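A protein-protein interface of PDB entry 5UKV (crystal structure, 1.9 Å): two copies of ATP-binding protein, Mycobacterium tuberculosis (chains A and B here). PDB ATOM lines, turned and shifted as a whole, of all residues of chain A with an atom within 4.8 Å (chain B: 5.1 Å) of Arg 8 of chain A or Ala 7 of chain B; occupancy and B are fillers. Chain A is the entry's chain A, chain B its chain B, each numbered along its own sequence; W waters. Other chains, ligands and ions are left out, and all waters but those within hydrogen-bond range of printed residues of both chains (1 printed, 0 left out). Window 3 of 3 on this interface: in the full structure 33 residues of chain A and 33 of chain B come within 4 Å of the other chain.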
ATOM      1  N   ALA A   4      15.627 -12.148 -11.787  1.00  0.00           N
ATOM      2  CA  ALA A   4      16.515 -12.028 -10.710  1.00  0.00           C
ATOM      3  C   ALA A   4      16.864 -10.547 -10.406  1.00  0.00           C
ATOM      4  O   ALA A   4      16.927 -10.096  -9.247  1.00  0.00           O
ATOM      5  CB  ALA A   4      17.788 -12.859 -10.948  1.00  0.00           C
ATOM      6  N   GLU A   5      17.079  -9.802 -11.453  1.00  0.00           N
ATOM      7  CA  GLU A   5      17.491  -8.460 -11.297  1.00  0.00           C
ATOM      8  C   GLU A   5      16.326  -7.667 -10.589  1.00  0.00           C
ATOM      9  O   GLU A   5      16.612  -6.887  -9.709  1.00  0.00           O
ATOM     10  CB  GLU A   5      17.773  -7.853 -12.655  1.00  0.00           C
ATOM     11  CG  GLU A   5      18.729  -6.694 -12.559  1.00  0.00           C
ATOM     12  CD  GLU A   5      18.577  -5.663 -13.661  1.00  0.00           C
ATOM     13  OE1 GLU A   5      18.742  -4.426 -13.356  1.00  0.00           O
ATOM     14  OE2 GLU A   5      18.309  -6.079 -14.833  1.00  0.00           O
ATOM     15  N   LYS A   6      15.088  -7.846 -11.003  1.00  0.00           N
ATOM     16  CA  LYS A   6      13.925  -7.126 -10.414  1.00  0.00           C
ATOM     17  C   LYS A   6      13.722  -7.567  -8.979  1.00  0.00           C
ATOM     18  O   LYS A   6      13.329  -6.784  -8.104  1.00  0.00           O
ATOM     19  CB  LYS A   6      12.634  -7.414 -11.177  1.00  0.00           C
ATOM     20  CG  LYS A   6      12.679  -6.848 -12.594  1.00  0.00           C
ATOM     21  CD  LYS A   6      11.433  -7.259 -13.381  1.00  0.00           C
ATOM     22  CE  LYS A   6      11.150  -6.337 -14.523  1.00  0.00           C
ATOM     23  NZ  LYS A   6       9.672  -6.302 -14.745  1.00  0.00           N
ATOM     24  N   ALA A   7      13.872  -8.863  -8.770  1.00  0.00           N
ATOM     25  CA  ALA A   7      13.760  -9.403  -7.471  1.00  0.00           C
ATOM     26  C   ALA A   7      14.821  -8.866  -6.471  1.00  0.00           C
ATOM     27  O   ALA A   7      14.502  -8.640  -5.316  1.00  0.00           O
ATOM     28  CB  ALA A   7      13.872 -10.894  -7.546  1.00  0.00           C
ATOM     29  N   ARG A   8      16.088  -8.776  -6.911  1.00  0.00           N
ATOM     30  CA  ARG A   8      17.136  -8.238  -6.113  1.00  0.00           C
ATOM     31  C   ARG A   8      16.922  -6.801  -5.835  1.00  0.00           C
ATOM     32  O   ARG A   8      17.263  -6.379  -4.771  1.00  0.00           O
ATOM     33  CB  ARG A   8      18.535  -8.401  -6.711  1.00  0.00           C
ATOM     34  CG  ARG A   8      19.157  -9.710  -6.361  1.00  0.00           C
ATOM     35  CD  ARG A   8      20.686  -9.725  -6.528  1.00  0.00           C
ATOM     36  NE  ARG A   8      21.014 -10.056  -7.929  1.00  0.00           N
ATOM     37  CZ  ARG A   8      21.432  -9.216  -8.895  1.00  0.00           C
ATOM     38  NH1 ARG A   8      21.661  -7.914  -8.673  1.00  0.00           N
ATOM     39  NH2 ARG A   8      21.624  -9.702 -10.106  1.00  0.00           N
ATOM     40  N   ASP A   9      16.471  -6.043  -6.825  1.00  0.00           N
ATOM     41  CA  ASP A   9      16.145  -4.664  -6.640  1.00  0.00           C
ATOM     42  C   ASP A   9      15.040  -4.512  -5.578  1.00  0.00           C
ATOM     43  O   ASP A   9      15.154  -3.698  -4.704  1.00  0.00           O
ATOM     44  CB  ASP A   9      15.698  -4.047  -7.884  1.00  0.00           C
ATOM     45  CG  ASP A   9      15.410  -2.531  -7.708  1.00  0.00           C
ATOM     46  OD1 ASP A   9      16.360  -1.759  -7.547  1.00  0.00           O
ATOM     47  OD2 ASP A   9      14.249  -2.097  -7.680  1.00  0.00           O
ATOM     48  N   SER A  10      14.036  -5.355  -5.626  1.00  0.00           N
ATOM     49  CA  SER A  10      12.992  -5.273  -4.647  1.00  0.00           C
ATOM     50  C   SER A  10      13.509  -5.632  -3.232  1.00  0.00           C
ATOM     51  O   SER A  10      13.263  -4.913  -2.211  1.00  0.00           O
ATOM     52  CB  SER A  10      11.853  -6.146  -5.128  1.00  0.00           C
ATOM     53  OG  SER A  10      10.831  -6.087  -4.186  1.00  0.00           O
ATOM     54  N   GLU A  11      14.328  -6.680  -3.159  1.00  0.00           N
ATOM     55  CA  GLU A  11      14.971  -7.047  -1.912  1.00  0.00           C
ATOM     56  C   GLU A  11      15.898  -5.936  -1.303  1.00  0.00           C
ATOM     57  O   GLU A  11      15.801  -5.662  -0.124  1.00  0.00           O
ATOM     58  CB  GLU A  11      15.718  -8.338  -2.071  1.00  0.00           C
ATOM     59  CG  GLU A  11      16.494  -8.708  -0.817  1.00  0.00           C
ATOM     60  CD  GLU A  11      17.605  -9.698  -0.999  1.00  0.00           C
ATOM     61  OE1 GLU A  11      18.091 -10.095   0.078  1.00  0.00           O
ATOM     62  OE2 GLU A  11      17.907 -10.124  -2.164  1.00  0.00           O
ATOM     63  N   ASP A  12      16.764  -5.322  -2.102  1.00  0.00           N
ATOM     64  CA  ASP A  12      17.559  -4.280  -1.656  1.00  0.00           C
ATOM     65  C   ASP A  12      16.757  -3.041  -1.226  1.00  0.00           C
ATOM     66  O   ASP A  12      17.119  -2.413  -0.287  1.00  0.00           O
ATOM     67  CB  ASP A  12      18.573  -3.863  -2.693  1.00  0.00           C
ATOM     68  CG  ASP A  12      19.690  -4.901  -2.844  1.00  0.00           C
ATOM     69  OD1 ASP A  12      19.734  -5.939  -2.091  1.00  0.00           O
ATOM     70  OD2 ASP A  12      20.460  -4.707  -3.790  1.00  0.00           O
ATOM     71  N   MET B   3      17.456 -17.692  -8.601  1.00  0.00           N
ATOM     72  CA  MET B   3      17.969 -16.452  -7.988  1.00  0.00           C
ATOM     73  C   MET B   3      16.815 -15.532  -7.608  1.00  0.00           C
ATOM     74  O   MET B   3      16.854 -14.966  -6.553  1.00  0.00           O
ATOM     75  CB  MET B   3      18.865 -15.609  -8.903  1.00  0.00           C
ATOM     76  CG  MET B   3      20.135 -16.322  -9.378  1.00  0.00           C
ATOM     77  SD  MET B   3      21.214 -16.810  -7.784  1.00  0.00           S
ATOM     78  CE  MET B   3      22.614 -17.923  -8.676  1.00  0.00           C
ATOM     79  N   ALA B   4      15.817 -15.397  -8.481  1.00  0.00           N
ATOM     80  CA  ALA B   4      14.592 -14.603  -8.193  1.00  0.00           C
ATOM     81  C   ALA B   4      13.851 -15.120  -6.940  1.00  0.00           C
ATOM     82  O   ALA B   4      13.416 -14.343  -6.103  1.00  0.00           O
ATOM     83  CB  ALA B   4      13.665 -14.559  -9.414  1.00  0.00           C
ATOM     84  N   GLU B   5      13.792 -16.447  -6.825  1.00  0.00           N
ATOM     85  CA  GLU B   5      13.259 -17.153  -5.673  1.00  0.00           C
ATOM     86  C   GLU B   5      13.988 -16.843  -4.352  1.00  0.00           C
ATOM     87  O   GLU B   5      13.349 -16.537  -3.360  1.00  0.00           O
ATOM     88  CB  GLU B   5      13.272 -18.708  -5.939  1.00  0.00           C
ATOM     89  CG  GLU B   5      12.891 -19.610  -4.736  1.00  0.00           C
ATOM     90  CD  GLU B   5      12.787 -21.113  -5.109  1.00  0.00           C
ATOM     91  OE1 GLU B   5      11.677 -21.699  -4.879  1.00  0.00           O
ATOM     92  OE2 GLU B   5      13.806 -21.682  -5.652  1.00  0.00           O
ATOM     93  N   LYS B   6      15.297 -17.006  -4.324  1.00  0.00           N
ATOM     94  CA  LYS B   6      16.066 -16.618  -3.156  1.00  0.00           C
ATOM     95  C   LYS B   6      15.840 -15.131  -2.747  1.00  0.00           C
ATOM     96  O   LYS B   6      15.641 -14.848  -1.593  1.00  0.00           O
ATOM     97  CB  LYS B   6      17.558 -16.872  -3.359  1.00  0.00           C
ATOM     98  CG  LYS B   6      18.015 -18.342  -3.217  1.00  0.00           C
ATOM     99  CD  LYS B   6      19.552 -18.475  -3.270  1.00  0.00           C
ATOM    100  CE  LYS B   6      20.253 -18.055  -1.960  1.00  0.00           C
ATOM    101  NZ  LYS B   6      21.639 -17.541  -2.182  1.00  0.00           N
ATOM    102  N   ALA B   7      15.907 -14.197  -3.682  1.00  0.00           N
ATOM    103  CA  ALA B   7      15.737 -12.798  -3.377  1.00  0.00           C
ATOM    104  C   ALA B   7      14.346 -12.563  -2.833  1.00  0.00           C
ATOM    105  O   ALA B   7      14.211 -11.808  -1.883  1.00  0.00           O
ATOM    106  CB  ALA B   7      15.975 -11.958  -4.571  1.00  0.00           C
ATOM    107  N   ARG B   8      13.353 -13.197  -3.420  1.00  0.00           N
ATOM    108  CA  ARG B   8      11.980 -13.113  -2.979  1.00  0.00           C
ATOM    109  C   ARG B   8      11.767 -13.731  -1.623  1.00  0.00           C
ATOM    110  O   ARG B   8      11.121 -13.177  -0.800  1.00  0.00           O
ATOM    111  CB  ARG B   8      11.079 -13.774  -3.970  1.00  0.00           C
ATOM    112  CG  ARG B   8       9.648 -13.680  -3.602  1.00  0.00           C
ATOM    113  CD  ARG B   8       9.279 -12.243  -3.489  1.00  0.00           C
ATOM    114  NE  ARG B   8       8.247 -12.101  -2.510  1.00  0.00           N
ATOM    115  CZ  ARG B   8       7.014 -11.759  -2.794  1.00  0.00           C
ATOM    116  NH1 ARG B   8       6.127 -11.663  -1.837  1.00  0.00           N
ATOM    117  NH2 ARG B   8       6.680 -11.535  -4.036  1.00  0.00           N
ATOM    118  N   ASP B   9      12.343 -14.898  -1.408  1.00  0.00           N
ATOM    119  CA  ASP B   9      12.288 -15.524  -0.097  1.00  0.00           C
ATOM    120  C   ASP B   9      12.927 -14.643   0.999  1.00  0.00           C
ATOM    121  O   ASP B   9      12.432 -14.529   2.152  1.00  0.00           O
ATOM    122  CB  ASP B   9      13.002 -16.891  -0.061  1.00  0.00           C
ATOM    123  CG  ASP B   9      13.011 -17.476   1.367  1.00  0.00           C
ATOM    124  OD1 ASP B   9      11.878 -17.756   1.867  1.00  0.00           O
ATOM    125  OD2 ASP B   9      14.108 -17.508   2.025  1.00  0.00           O
ATOM    126  N   SER B  10      14.032 -14.014   0.638  1.00  0.00           N
ATOM    127  CA  SER B  10      14.726 -13.099   1.538  1.00  0.00           C
ATOM    128  C   SER B  10      13.864 -11.867   1.882  1.00  0.00           C
ATOM    129  O   SER B  10      13.698 -11.515   3.045  1.00  0.00           O
ATOM    130  CB  SER B  10      15.975 -12.668   0.877  1.00  0.00           C
ATOM    131  OG  SER B  10      16.651 -11.811   1.694  1.00  0.00           O
ATOM    132  N   GLU B  11      13.276 -11.255   0.894  1.00  0.00           N
ATOM    133  CA  GLU B  11      12.322 -10.104   1.081  1.00  0.00           C
ATOM    134  C   GLU B  11      11.083 -10.423   1.938  1.00  0.00           C
ATOM    135  O   GLU B  11      10.703  -9.693   2.811  1.00  0.00           O
ATOM    136  CB  GLU B  11      11.883  -9.556  -0.299  1.00  0.00           C
ATOM    137  CG  GLU B  11      10.993  -8.351  -0.211  1.00  0.00           C
ATOM    138  CD  GLU B  11      10.227  -8.011  -1.485  1.00  0.00           C
ATOM    139  OE1 GLU B  11       8.975  -7.840  -1.412  1.00  0.00           O
ATOM    140  OE2 GLU B  11      10.878  -8.000  -2.569  1.00  0.00           O
HETATM  141  O   HOH W   1      12.174  -9.870  -4.269  1.00  0.00           O
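The side-chain hydroxyl (OG) of Ser 10 of chain A is in hydrogen-bond range of the side-chain carboxylate (OE2) of Glu 11 of chain B, 2.5 Å away. The side-chain carboxylate (OE1) of Glu 11 of chain A sits at hydrogen-bond distance from the side-chain hydroxyl (OG) of Ser 10 of chain B (2.8 Å).
CB of Ala 4 of chain A touches CB of Met 3 of chain B, at 3.6 Å. Ala 4 of chain B touches Ala 4 of chain A. Ala 7 of chain A touches Ala 4 of chain B (CB to O, 3.8 Å). CB of Ala 7 of chain B touches O of Ala 7 of chain A (3.7 Å). Arg 8 of chain A touches Ala 7 of chain B (N to CB, 3.95 Å). Glu 11 of chain A touches Ala 7 of chain B. Glu 11 of chain B touches Glu 11 of chain A.
Arg 8 of chain A touches one residue of chain B. Printed residues of chain A within 4 Å of Glu 11 of chain B: Ser 10 (2.5 Å) and Glu 11 (3.7 Å). Printed residues of chain A within 4 Å of Met 3 of chain B: Ala 4. Of the printed residues of chain A, Ser 10 of chain B touches Glu 11 (2.8 Å). Of the printed residues of chain A, Ala 4 of chain B touches Ala 4 (3.9 Å) and Ala 7 (3.8 Å). Of the printed residues of chain B, Ser 10 of chain A touches Glu 11 (2.5 Å). The nearest printed residue of chain B that does not touch Arg 8 of chain A is Met 3 of chain B (5.7 Å). The nearest printed residue of chain A that does not touch Ala 7 of chain B is Ala 4 of chain A (5.1 Å).
Of the 9 printed residues of chain A, 5 touch a printed residue of chain B. Hydrophobic or aromatic side chains of chain A that line the printed part of chain B: Ala 4 and Ala 7. Hydrophobic or aromatic side chains of chain B within 4 Å of the printed part of chain A: Met 3, Ala 4 and Ala 7. Among the printed residues, no Asp or Glu carboxylate lies within 4 Å of a Lys or Arg side-chain nitrogen of the other chain.
Ala 7 of chain A touches Ala 4 of chain B, but with the chains exchanged Ala 4 of chain A does not touch Ala 7 of chain B (5.1 Å). Ala 7 of chain A touches its own counterpart, Ala 7 of chain B. Ser 10 of chain A touches Glu 11 of chain B, and with the chains exchanged Glu 11 of chain A touches Ser 10 of chain B. Glu 11 of chain A touches Ala 7 of chain B, but with the chains exchanged Ala 7 of chain A does not touch Glu 11 of chain B (4.6 Å).
Water W1 lies within hydrogen-bond range of the backbone carbonyl oxygen (O) of Ala 7 of chain A (2.8 Å) and the side-chain carboxylate (OE2) of Glu 11 of chain B (2.8 Å).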
